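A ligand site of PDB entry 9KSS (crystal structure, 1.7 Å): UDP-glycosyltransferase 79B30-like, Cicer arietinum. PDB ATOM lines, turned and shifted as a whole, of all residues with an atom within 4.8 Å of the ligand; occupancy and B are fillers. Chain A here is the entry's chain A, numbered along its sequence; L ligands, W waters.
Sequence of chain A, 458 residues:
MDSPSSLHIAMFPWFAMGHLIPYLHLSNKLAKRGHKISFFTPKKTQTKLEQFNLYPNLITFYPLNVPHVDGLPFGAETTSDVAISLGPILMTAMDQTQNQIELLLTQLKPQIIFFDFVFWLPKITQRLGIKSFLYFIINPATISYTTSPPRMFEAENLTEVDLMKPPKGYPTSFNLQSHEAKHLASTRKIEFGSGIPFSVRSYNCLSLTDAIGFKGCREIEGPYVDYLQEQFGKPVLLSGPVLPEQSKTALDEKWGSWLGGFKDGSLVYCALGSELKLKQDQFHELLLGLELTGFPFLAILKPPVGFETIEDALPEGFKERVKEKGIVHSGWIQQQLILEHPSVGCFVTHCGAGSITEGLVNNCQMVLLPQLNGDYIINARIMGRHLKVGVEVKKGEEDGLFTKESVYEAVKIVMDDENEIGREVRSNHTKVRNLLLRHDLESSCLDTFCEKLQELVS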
ATOM      1  N   TRP A  14     -13.272  -4.884 -12.298  1.00  0.00           N
ATOM      2  CA  TRP A  14     -12.753  -3.595 -11.849  1.00  0.00           C
ATOM      3  C   TRP A  14     -11.341  -3.381 -12.377  1.00  0.00           C
ATOM      4  O   TRP A  14     -10.596  -4.333 -12.623  1.00  0.00           O
ATOM      5  CB  TRP A  14     -12.804  -3.569 -10.312  1.00  0.00           C
ATOM      6  CG  TRP A  14     -12.042  -2.509  -9.526  1.00  0.00           C
ATOM      7  CD1 TRP A  14     -11.206  -2.743  -8.468  1.00  0.00           C
ATOM      8  CD2 TRP A  14     -12.152  -1.087  -9.649  1.00  0.00           C
ATOM      9  NE1 TRP A  14     -10.735  -1.550  -7.956  1.00  0.00           N
ATOM     10  CE2 TRP A  14     -11.307  -0.519  -8.656  1.00  0.00           C
ATOM     11  CE3 TRP A  14     -12.828  -0.226 -10.525  1.00  0.00           C
ATOM     12  CZ2 TRP A  14     -11.146   0.862  -8.504  1.00  0.00           C
ATOM     13  CZ3 TRP A  14     -12.657   1.155 -10.370  1.00  0.00           C
ATOM     14  CH2 TRP A  14     -11.825   1.685  -9.364  1.00  0.00           C
ATOM     15  N   ALA A  16      -8.218  -3.046 -11.776  1.00  0.00           N
ATOM     16  CA  ALA A  16      -7.205  -3.327 -10.768  1.00  0.00           C
ATOM     17  C   ALA A  16      -6.559  -4.649 -11.137  1.00  0.00           C
ATOM     18  O   ALA A  16      -7.230  -5.565 -11.615  1.00  0.00           O
ATOM     19  CB  ALA A  16      -7.831  -3.400  -9.368  1.00  0.00           C
ATOM     20  N   HIS A  19      -8.002  -7.801  -9.732  1.00  0.00           N
ATOM     21  CA  HIS A  19      -9.237  -8.305 -10.313  1.00  0.00           C
ATOM     22  C   HIS A  19      -9.018  -8.816 -11.731  1.00  0.00           C
ATOM     23  O   HIS A  19      -9.501  -9.899 -12.061  1.00  0.00           O
ATOM     24  CB  HIS A  19     -10.311  -7.203 -10.311  1.00  0.00           C
ATOM     25  CG  HIS A  19     -10.728  -6.791  -8.928  1.00  0.00           C
ATOM     26  ND1 HIS A  19     -12.041  -6.860  -8.501  1.00  0.00           N
ATOM     27  CD2 HIS A  19     -10.013  -6.341  -7.874  1.00  0.00           C
ATOM     28  CE1 HIS A  19     -12.100  -6.481  -7.239  1.00  0.00           C
ATOM     29  NE2 HIS A  19     -10.885  -6.152  -6.836  1.00  0.00           N
ATOM     30  N   THR A  79      -5.844   0.795 -10.654  1.00  0.00           N
ATOM     31  CA  THR A  79      -5.475   1.264  -9.324  1.00  0.00           C
ATOM     32  C   THR A  79      -3.973   1.224  -9.108  1.00  0.00           C
ATOM     33  O   THR A  79      -3.475   1.850  -8.164  1.00  0.00           O
ATOM     34  CB  THR A  79      -6.160   0.435  -8.239  1.00  0.00           C
ATOM     35  OG1 THR A  79      -5.827  -0.946  -8.430  1.00  0.00           O
ATOM     36  CG2 THR A  79      -7.688   0.638  -8.253  1.00  0.00           C
ATOM     37  N   ILE A  84      -4.160   5.321  -3.578  1.00  0.00           N
ATOM     38  CA  ILE A  84      -5.391   4.696  -3.100  1.00  0.00           C
ATOM     39  C   ILE A  84      -6.487   5.738  -2.929  1.00  0.00           C
ATOM     40  O   ILE A  84      -7.661   5.470  -3.202  1.00  0.00           O
ATOM     41  CB  ILE A  84      -5.142   3.910  -1.790  1.00  0.00           C
ATOM     42  CG1 ILE A  84      -6.451   3.496  -1.147  1.00  0.00           C
ATOM     43  CG2 ILE A  84      -4.385   4.761  -0.793  1.00  0.00           C
ATOM     44  CD1 ILE A  84      -7.223   2.526  -1.967  1.00  0.00           C
ATOM     45  N   PHE A 115     -19.182  -9.119 -13.647  1.00  0.00           N
ATOM     46  CA  PHE A 115     -18.821  -7.716 -13.427  1.00  0.00           C
ATOM     47  C   PHE A 115     -18.488  -7.444 -11.964  1.00  0.00           C
ATOM     48  O   PHE A 115     -18.889  -8.185 -11.061  1.00  0.00           O
ATOM     49  CB  PHE A 115     -19.944  -6.776 -13.902  1.00  0.00           C
ATOM     50  CG  PHE A 115     -21.156  -6.746 -13.001  1.00  0.00           C
ATOM     51  CD1 PHE A 115     -22.092  -7.778 -13.039  1.00  0.00           C
ATOM     52  CD2 PHE A 115     -21.388  -5.681 -12.117  1.00  0.00           C
ATOM     53  CE1 PHE A 115     -23.213  -7.771 -12.214  1.00  0.00           C
ATOM     54  CE2 PHE A 115     -22.515  -5.658 -11.306  1.00  0.00           C
ATOM     55  CZ  PHE A 115     -23.429  -6.711 -11.349  1.00  0.00           C
ATOM     56  N   ASP A 116     -17.741  -6.355 -11.745  1.00  0.00           N
ATOM     57  CA  ASP A 116     -17.581  -5.660 -10.470  1.00  0.00           C
ATOM     58  C   ASP A 116     -18.268  -4.306 -10.431  1.00  0.00           C
ATOM     59  O   ASP A 116     -18.306  -3.616 -11.437  1.00  0.00           O
ATOM     60  CB  ASP A 116     -16.107  -5.369 -10.118  1.00  0.00           C
ATOM     61  CG  ASP A 116     -15.280  -6.593  -9.839  1.00  0.00           C
ATOM     62  OD1 ASP A 116     -15.628  -7.274  -8.854  1.00  0.00           O
ATOM     63  OD2 ASP A 116     -14.216  -6.796 -10.449  1.00  0.00           O
ATOM     64  N   PHE A 117     -18.780  -3.924  -9.252  1.00  0.00           N
ATOM     65  CA  PHE A 117     -19.021  -2.523  -8.888  1.00  0.00           C
ATOM     66  C   PHE A 117     -20.111  -1.751  -9.638  1.00  0.00           C
ATOM     67  O   PHE A 117     -20.706  -0.852  -9.045  1.00  0.00           O
ATOM     68  CB  PHE A 117     -17.724  -1.708  -9.035  1.00  0.00           C
ATOM     69  CG  PHE A 117     -16.770  -1.806  -7.861  1.00  0.00           C
ATOM     70  CD1 PHE A 117     -17.217  -1.677  -6.548  1.00  0.00           C
ATOM     71  CD2 PHE A 117     -15.406  -1.956  -8.094  1.00  0.00           C
ATOM     72  CE1 PHE A 117     -16.325  -1.724  -5.492  1.00  0.00           C
ATOM     73  CE2 PHE A 117     -14.497  -2.025  -7.030  1.00  0.00           C
ATOM     74  CZ  PHE A 117     -14.951  -1.916  -5.729  1.00  0.00           C
ATOM     75  N   LEU A 134     -22.619 -10.872 -10.705  1.00  0.00           N
ATOM     76  CA  LEU A 134     -21.674 -10.106  -9.894  1.00  0.00           C
ATOM     77  C   LEU A 134     -20.601 -11.073  -9.383  1.00  0.00           C
ATOM     78  O   LEU A 134     -20.896 -11.918  -8.541  1.00  0.00           O
ATOM     79  CB  LEU A 134     -22.428  -9.443  -8.757  1.00  0.00           C
ATOM     80  CG  LEU A 134     -21.655  -8.704  -7.669  1.00  0.00           C
ATOM     81  CD1 LEU A 134     -20.903  -7.495  -8.248  1.00  0.00           C
ATOM     82  CD2 LEU A 134     -22.651  -8.250  -6.608  1.00  0.00           C
ATOM     83  N   PHE A 136     -17.160 -11.766  -7.475  1.00  0.00           N
ATOM     84  CA  PHE A 136     -16.181 -11.240  -6.521  1.00  0.00           C
ATOM     85  C   PHE A 136     -14.930 -12.103  -6.473  1.00  0.00           C
ATOM     86  O   PHE A 136     -15.024 -13.328  -6.306  1.00  0.00           O
ATOM     87  CB  PHE A 136     -16.747 -11.227  -5.107  1.00  0.00           C
ATOM     88  CG  PHE A 136     -17.874 -10.275  -4.861  1.00  0.00           C
ATOM     89  CD1 PHE A 136     -17.640  -8.943  -4.550  1.00  0.00           C
ATOM     90  CD2 PHE A 136     -19.180 -10.715  -4.942  1.00  0.00           C
ATOM     91  CE1 PHE A 136     -18.687  -8.076  -4.296  1.00  0.00           C
ATOM     92  CE2 PHE A 136     -20.231  -9.864  -4.677  1.00  0.00           C
ATOM     93  CZ  PHE A 136     -19.988  -8.541  -4.358  1.00  0.00           C
ATOM     94  N   ILE A 138     -12.825 -11.105  -3.962  1.00  0.00           N
ATOM     95  CA  ILE A 138     -12.553 -10.884  -2.551  1.00  0.00           C
ATOM     96  C   ILE A 138     -13.283 -11.952  -1.755  1.00  0.00           C
ATOM     97  O   ILE A 138     -14.058 -12.746  -2.300  1.00  0.00           O
ATOM     98  CB  ILE A 138     -12.974  -9.472  -2.084  1.00  0.00           C
ATOM     99  CG1 ILE A 138     -14.477  -9.276  -2.240  1.00  0.00           C
ATOM    100  CG2 ILE A 138     -12.218  -8.393  -2.857  1.00  0.00           C
ATOM    101  CD1 ILE A 138     -15.017  -8.139  -1.356  1.00  0.00           C
ATOM    102  N   THR A 142     -15.913 -11.115   3.847  1.00  0.00           N
ATOM    103  CA  THR A 142     -15.849  -9.664   3.897  1.00  0.00           C
ATOM    104  C   THR A 142     -17.187  -9.049   3.519  1.00  0.00           C
ATOM    105  O   THR A 142     -17.766  -8.275   4.289  1.00  0.00           O
ATOM    106  CB  THR A 142     -14.742  -9.190   2.955  1.00  0.00           C
ATOM    107  OG1 THR A 142     -13.507  -9.792   3.375  1.00  0.00           O
ATOM    108  CG2 THR A 142     -14.596  -7.655   2.971  1.00  0.00           C
ATOM    109  N   ILE A 143     -17.704  -9.420   2.335  1.00  0.00           N
ATOM    110  CA  ILE A 143     -19.014  -8.927   1.917  1.00  0.00           C
ATOM    111  C   ILE A 143     -20.089  -9.242   2.950  1.00  0.00           C
ATOM    112  O   ILE A 143     -20.924  -8.400   3.260  1.00  0.00           O
ATOM    113  CB  ILE A 143     -19.371  -9.489   0.532  1.00  0.00           C
ATOM    114  CG1 ILE A 143     -18.479  -8.845  -0.528  1.00  0.00           C
ATOM    115  CG2 ILE A 143     -20.871  -9.295   0.236  1.00  0.00           C
ATOM    116  CD1 ILE A 143     -18.655  -7.306  -0.628  1.00  0.00           C
ATOM    117  N   THR A 146     -19.819  -6.756   6.028  1.00  0.00           N
ATOM    118  CA  THR A 146     -19.988  -5.319   5.892  1.00  0.00           C
ATOM    119  C   THR A 146     -21.191  -4.897   5.078  1.00  0.00           C
ATOM    120  O   THR A 146     -21.675  -3.771   5.239  1.00  0.00           O
ATOM    121  CB  THR A 146     -18.743  -4.690   5.235  1.00  0.00           C
ATOM    122  OG1 THR A 146     -18.603  -5.246   3.923  1.00  0.00           O
ATOM    123  CG2 THR A 146     -17.500  -4.984   6.062  1.00  0.00           C
ATOM    124  N   THR A 147     -21.715  -5.779   4.223  1.00  0.00           N
ATOM    125  CA  THR A 147     -22.670  -5.387   3.195  1.00  0.00           C
ATOM    126  C   THR A 147     -23.918  -6.278   3.180  1.00  0.00           C
ATOM    127  O   THR A 147     -24.711  -6.201   2.228  1.00  0.00           O
ATOM    128  CB  THR A 147     -21.970  -5.382   1.825  1.00  0.00           C
ATOM    129  OG1 THR A 147     -20.637  -4.836   1.972  1.00  0.00           O
ATOM    130  CG2 THR A 147     -22.748  -4.562   0.778  1.00  0.00           C
ATOM    131  N   PHE A 192     -17.583   6.498  -3.378  1.00  0.00           N
ATOM    132  CA  PHE A 192     -16.693   5.721  -4.240  1.00  0.00           C
ATOM    133  C   PHE A 192     -17.294   5.735  -5.639  1.00  0.00           C
ATOM    134  O   PHE A 192     -18.004   4.808  -6.039  1.00  0.00           O
ATOM    135  CB  PHE A 192     -16.530   4.285  -3.708  1.00  0.00           C
ATOM    136  CG  PHE A 192     -15.471   3.496  -4.419  1.00  0.00           C
ATOM    137  CD1 PHE A 192     -14.131   3.746  -4.195  1.00  0.00           C
ATOM    138  CD2 PHE A 192     -15.821   2.496  -5.321  1.00  0.00           C
ATOM    139  CE1 PHE A 192     -13.148   2.990  -4.846  1.00  0.00           C
ATOM    140  CE2 PHE A 192     -14.848   1.741  -5.975  1.00  0.00           C
ATOM    141  CZ  PHE A 192     -13.510   1.996  -5.743  1.00  0.00           C
ATOM    142  N   PHE A 198     -19.480   3.981  -0.552  1.00  0.00           N
ATOM    143  CA  PHE A 198     -18.828   2.721  -0.903  1.00  0.00           C
ATOM    144  C   PHE A 198     -19.725   1.505  -0.648  1.00  0.00           C
ATOM    145  O   PHE A 198     -19.994   0.737  -1.570  1.00  0.00           O
ATOM    146  CB  PHE A 198     -17.504   2.601  -0.140  1.00  0.00           C
ATOM    147  CG  PHE A 198     -16.716   1.353  -0.455  1.00  0.00           C
ATOM    148  CD1 PHE A 198     -16.125   1.179  -1.687  1.00  0.00           C
ATOM    149  CD2 PHE A 198     -16.541   0.376   0.521  1.00  0.00           C
ATOM    150  CE1 PHE A 198     -15.402   0.034  -1.981  1.00  0.00           C
ATOM    151  CE2 PHE A 198     -15.812  -0.772   0.243  1.00  0.00           C
ATOM    152  CZ  PHE A 198     -15.234  -0.941  -1.021  1.00  0.00           C
ATOM    153  N   SER A 199     -20.227   1.331   0.577  1.00  0.00           N
ATOM    154  CA  SER A 199     -21.035   0.130   0.842  1.00  0.00           C
ATOM    155  C   SER A 199     -22.369   0.165   0.116  1.00  0.00           C
ATOM    156  O   SER A 199     -22.866  -0.888  -0.279  1.00  0.00           O
ATOM    157  CB  SER A 199     -21.243  -0.084   2.334  1.00  0.00           C
ATOM    158  OG  SER A 199     -20.011  -0.456   2.949  1.00  0.00           O
ATOM    159  N   SER A 202     -21.848  -1.447  -3.389  1.00  0.00           N
ATOM    160  CA  SER A 202     -21.792  -2.892  -3.466  1.00  0.00           C
ATOM    161  C   SER A 202     -23.125  -3.514  -3.117  1.00  0.00           C
ATOM    162  O   SER A 202     -23.517  -4.541  -3.688  1.00  0.00           O
ATOM    163  CB  SER A 202     -20.702  -3.432  -2.536  1.00  0.00           C
ATOM    164  OG  SER A 202     -19.428  -3.090  -3.081  1.00  0.00           O
ATOM    165  N   CYS A 205     -25.235  -3.479  -6.120  1.00  0.00           N
ATOM    166  CA  CYS A 205     -24.857  -4.568  -7.016  1.00  0.00           C
ATOM    167  C   CYS A 205     -25.461  -5.881  -6.540  1.00  0.00           C
ATOM    168  O   CYS A 205     -26.019  -6.650  -7.336  1.00  0.00           O
ATOM    169  CB  CYS A 205     -23.329  -4.683  -7.121  1.00  0.00           C
ATOM    170  SG  CYS A 205     -22.449  -3.306  -7.916  1.00  0.00           S
ATOM    171  N   GLU A 275      -1.004  -1.997  -5.175  1.00  0.00           N
ATOM    172  CA  GLU A 275      -1.787  -0.784  -5.011  1.00  0.00           C
ATOM    173  C   GLU A 275      -1.227   0.156  -3.962  1.00  0.00           C
ATOM    174  O   GLU A 275      -1.204   1.373  -4.177  1.00  0.00           O
ATOM    175  CB  GLU A 275      -3.234  -1.119  -4.641  1.00  0.00           C
ATOM    176  CG  GLU A 275      -4.000  -1.872  -5.678  1.00  0.00           C
ATOM    177  CD  GLU A 275      -5.432  -2.188  -5.243  1.00  0.00           C
ATOM    178  OE1 GLU A 275      -6.356  -1.729  -5.930  1.00  0.00           O
ATOM    179  OE2 GLU A 275      -5.644  -2.826  -4.181  1.00  0.00           O
ATOM    180  N   ASN A 373      -7.644  -2.424   5.093  1.00  0.00           N
ATOM    181  CA  ASN A 373      -8.642  -2.711   4.066  1.00  0.00           C
ATOM    182  C   ASN A 373      -9.435  -3.887   4.609  1.00  0.00           C
ATOM    183  O   ASN A 373      -8.830  -4.806   5.180  1.00  0.00           O
ATOM    184  CB  ASN A 373      -7.936  -3.018   2.733  1.00  0.00           C
ATOM    185  CG  ASN A 373      -8.836  -3.717   1.700  1.00  0.00           C
ATOM    186  OD1 ASN A 373      -9.296  -4.846   1.899  1.00  0.00           O
ATOM    187  ND2 ASN A 373      -9.051  -3.063   0.578  1.00  0.00           N
ATOM    188  N   GLY A 374     -10.770  -3.833   4.512  1.00  0.00           N
ATOM    189  CA  GLY A 374     -11.591  -4.870   5.135  1.00  0.00           C
ATOM    190  C   GLY A 374     -11.266  -6.279   4.681  1.00  0.00           C
ATOM    191  O   GLY A 374     -11.225  -7.228   5.488  1.00  0.00           O
ATOM    192  N   ASP A 375     -11.031  -6.464   3.387  1.00  0.00           N
ATOM    193  CA  ASP A 375     -10.749  -7.812   2.902  1.00  0.00           C
ATOM    194  C   ASP A 375      -9.398  -8.316   3.402  1.00  0.00           C
ATOM    195  O   ASP A 375      -9.279  -9.477   3.801  1.00  0.00           O
ATOM    196  CB  ASP A 375     -10.846  -7.864   1.376  1.00  0.00           C
ATOM    197  CG  ASP A 375     -10.938  -9.299   0.858  1.00  0.00           C
ATOM    198  OD1 ASP A 375     -11.905  -9.996   1.221  1.00  0.00           O
ATOM    199  OD2 ASP A 375     -10.057  -9.728   0.059  1.00  0.00           O
HETATM  200  C1  LIG L   1     -17.359  -4.874  -5.111  1.00  0.00           C
HETATM  201  C2  LIG L   1     -16.701  -4.615  -3.923  1.00  0.00           C
HETATM  202  C3  LIG L   1     -15.326  -4.867  -3.792  1.00  0.00           C
HETATM  203  C4  LIG L   1     -14.672  -4.622  -2.504  1.00  0.00           C
HETATM  204  C5  LIG L   1     -13.310  -4.595  -2.218  1.00  0.00           C
HETATM  205  C6  LIG L   1     -13.861  -4.303   0.152  1.00  0.00           C
HETATM  206  C7  LIG L   1     -15.865  -4.021   2.062  1.00  0.00           C
HETATM  207  C8  LIG L   1     -15.213  -4.352  -0.178  1.00  0.00           C
HETATM  208  C9  LIG L   1     -10.699  -3.560  -4.580  1.00  0.00           C
HETATM  209  C10 LIG L   1     -10.991  -1.276  -2.828  1.00  0.00           C
HETATM  210  C11 LIG L   1     -11.682  -0.005  -2.404  1.00  0.00           C
HETATM  211  C12 LIG L   1     -14.661  -5.484  -4.856  1.00  0.00           C
HETATM  212  C13 LIG L   1     -13.526  -4.103   1.516  1.00  0.00           C
HETATM  213  C14 LIG L   1     -14.519  -3.974   2.457  1.00  0.00           C
HETATM  214  C15 LIG L   1     -16.230  -4.227   0.734  1.00  0.00           C
HETATM  215  C16 LIG L   1     -11.448  -3.566  -3.260  1.00  0.00           C
HETATM  216  C17 LIG L   1      -9.612  -2.484  -4.528  1.00  0.00           C
HETATM  217  C18 LIG L   1     -10.158  -1.125  -4.099  1.00  0.00           C
HETATM  218  C19 LIG L   1     -15.330  -5.764  -6.043  1.00  0.00           C
HETATM  219  C20 LIG L   1     -16.673  -5.455  -6.173  1.00  0.00           C
HETATM  220  C21 LIG L   1     -12.881  -4.423  -0.901  1.00  0.00           C
HETATM  221  O1  LIG L   1     -11.656  -4.414  -0.608  1.00  0.00           O
HETATM  222  O2  LIG L   1     -10.086  -4.822  -4.772  1.00  0.00           O
HETATM  223  O3  LIG L   1     -18.686  -4.576  -5.267  1.00  0.00           O
HETATM  224  O4  LIG L   1     -17.387  -5.723  -7.303  1.00  0.00           O
HETATM  225  O5  LIG L   1     -15.583  -4.539  -1.483  1.00  0.00           O
HETATM  226  O6  LIG L   1     -16.832  -3.847   2.986  1.00  0.00           O
HETATM  227  O7  LIG L   1     -12.237  -4.061   1.889  1.00  0.00           O
HETATM  228  O8  LIG L   1     -12.405  -4.626  -3.255  1.00  0.00           O
HETATM  229  O9  LIG L   1     -12.012  -2.289  -3.016  1.00  0.00           O
HETATM  230  O10 LIG L   1     -10.724   0.982  -2.043  1.00  0.00           O
HETATM  231  O11 LIG L   1     -10.940  -0.528  -5.143  1.00  0.00           O
HETATM  232  O12 LIG L   1      -8.938  -2.416  -5.785  1.00  0.00           O
HETATM  233  O   HOH W   1      -7.302  -5.008  -5.788  1.00  0.00           O
HETATM  234  O   HOH W   2      -8.277  -5.337  -2.959  1.00  0.00           O
HETATM  235  O   HOH W   3     -19.140  -2.696   1.568  1.00  0.00           O
HETATM  236  O   HOH W   4      -9.702   1.944  -5.145  1.00  0.00           O
HETATM  237  O   HOH W   5     -16.866  -1.406   4.164  1.00  0.00           O
HETATM  238  O   HOH W   6     -11.807  -1.259   3.551  1.00  0.00           O
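An oxygen (O4) of the ligand sits at hydrogen-bond distance from the side-chain carboxylate (OD1) of Asp 116 (2.8 Å).
N of Gly 374 is in hydrogen-bond range of O7 of the ligand (3.0 Å).
An oxygen (O4) of the ligand lies within hydrogen-bond range of the backbone NH of Phe 117.
An oxygen (O2) of the ligand is in hydrogen-bond range of a ring nitrogen (NE2) of His 19 (2.6 Å).
An oxygen (O12) of the ligand is in hydrogen-bond range of the indole nitrogen of Trp 14.
The side-chain amide oxygen (OD1) of Asn 373 is in hydrogen-bond range of an oxygen (O7) of the ligand.
The side-chain hydroxyl (OG1) of Thr 146 is in hydrogen-bond range of an oxygen (O6) of the ligand (2.4 Å).
OE1 of Glu 275 is in hydrogen-bond range of O12 of the ligand (2.7 Å).
O7 of the ligand is in hydrogen-bond range of N of Asp 375 (3.1 Å).
OG of Ser 202 lies within hydrogen-bond range of O3 of the ligand (2.7 Å).
N of Asp 375 lies within hydrogen-bond range of OD1 of Asn 373.
The backbone NH (N) of Trp 14 lies within hydrogen-bond range of the side-chain carboxylate (OD2) of Asp 116.
O of Thr 142 sits at hydrogen-bond distance from OG1 of Thr 146.
A ring nitrogen (ND1) of His 19 sits at hydrogen-bond distance from the side-chain carboxylate of Asp 116 (2.9 Å).
The side-chain hydroxyl (OG1) of Thr 79 sits at hydrogen-bond distance from the side-chain carboxylate (OE1) of Glu 275, 2.7 Å away.
The side-chain hydroxyl (OG1) of Thr 146 lies within hydrogen-bond range of the side-chain hydroxyl (OG1) of Thr 147 (2.8 Å).
The side-chain sulfur of Cys 205 lies within hydrogen-bond range of the backbone carbonyl oxygen of Phe 117 (3.2 Å).
The side-chain carboxylate (OD1) of Asp 375 is in hydrogen-bond range of the side-chain hydroxyl (OG1) of Thr 142, 2.7 Å away.
Ala 16 touches the ligand.
Ile 84 touches the ligand (CD1 to O10, 3.8 Å).
Phe 136 touches the ligand.
CD1 of Ile 138 touches O5 of the ligand (3.6 Å).
Thr 142 touches the ligand (CG2 to C14, 3.7 Å).
Phe 192 touches the ligand (CZ to O11, 3.7 Å).
Phe 198 touches the ligand (CZ to C8, 3.5 Å).
Hydrophobic or aromatic side chains within 4 Å of the ligand: Trp 14, Ala 16, His 19, Ile 84, Phe 117, Phe 136, Ile 138, Phe 192 and Phe 198.
17 residues have an atom within 4 Å of the ligand: Trp 14, Ala 16, His 19, Ile 84, Asp 116, Phe 117, Phe 136, Ile 138, Thr 142, Thr 146, Phe 192, Phe 198, Ser 202, Glu 275, Asn 373, Gly 374 and Asp 375.
The nearest printed residue that does not touch the ligand is Leu 134 (4.05 Å).
Water W3 lies within hydrogen-bond range of the side-chain hydroxyl (OG1) of Thr 147 (2.6 Å), the side-chain hydroxyl (OG) of Ser 199 (2.8 Å) and an oxygen (O6) of the ligand (2.9 Å).
Water W1 bridges O2 of the ligand (3.0 Å) and OE2 of Glu 275 (3.2 Å).
Water W6 lies within hydrogen-bond range of the backbone NH (N) of Gly 374 (2.9 Å) and an oxygen (O7) of the ligand (3.3 Å).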
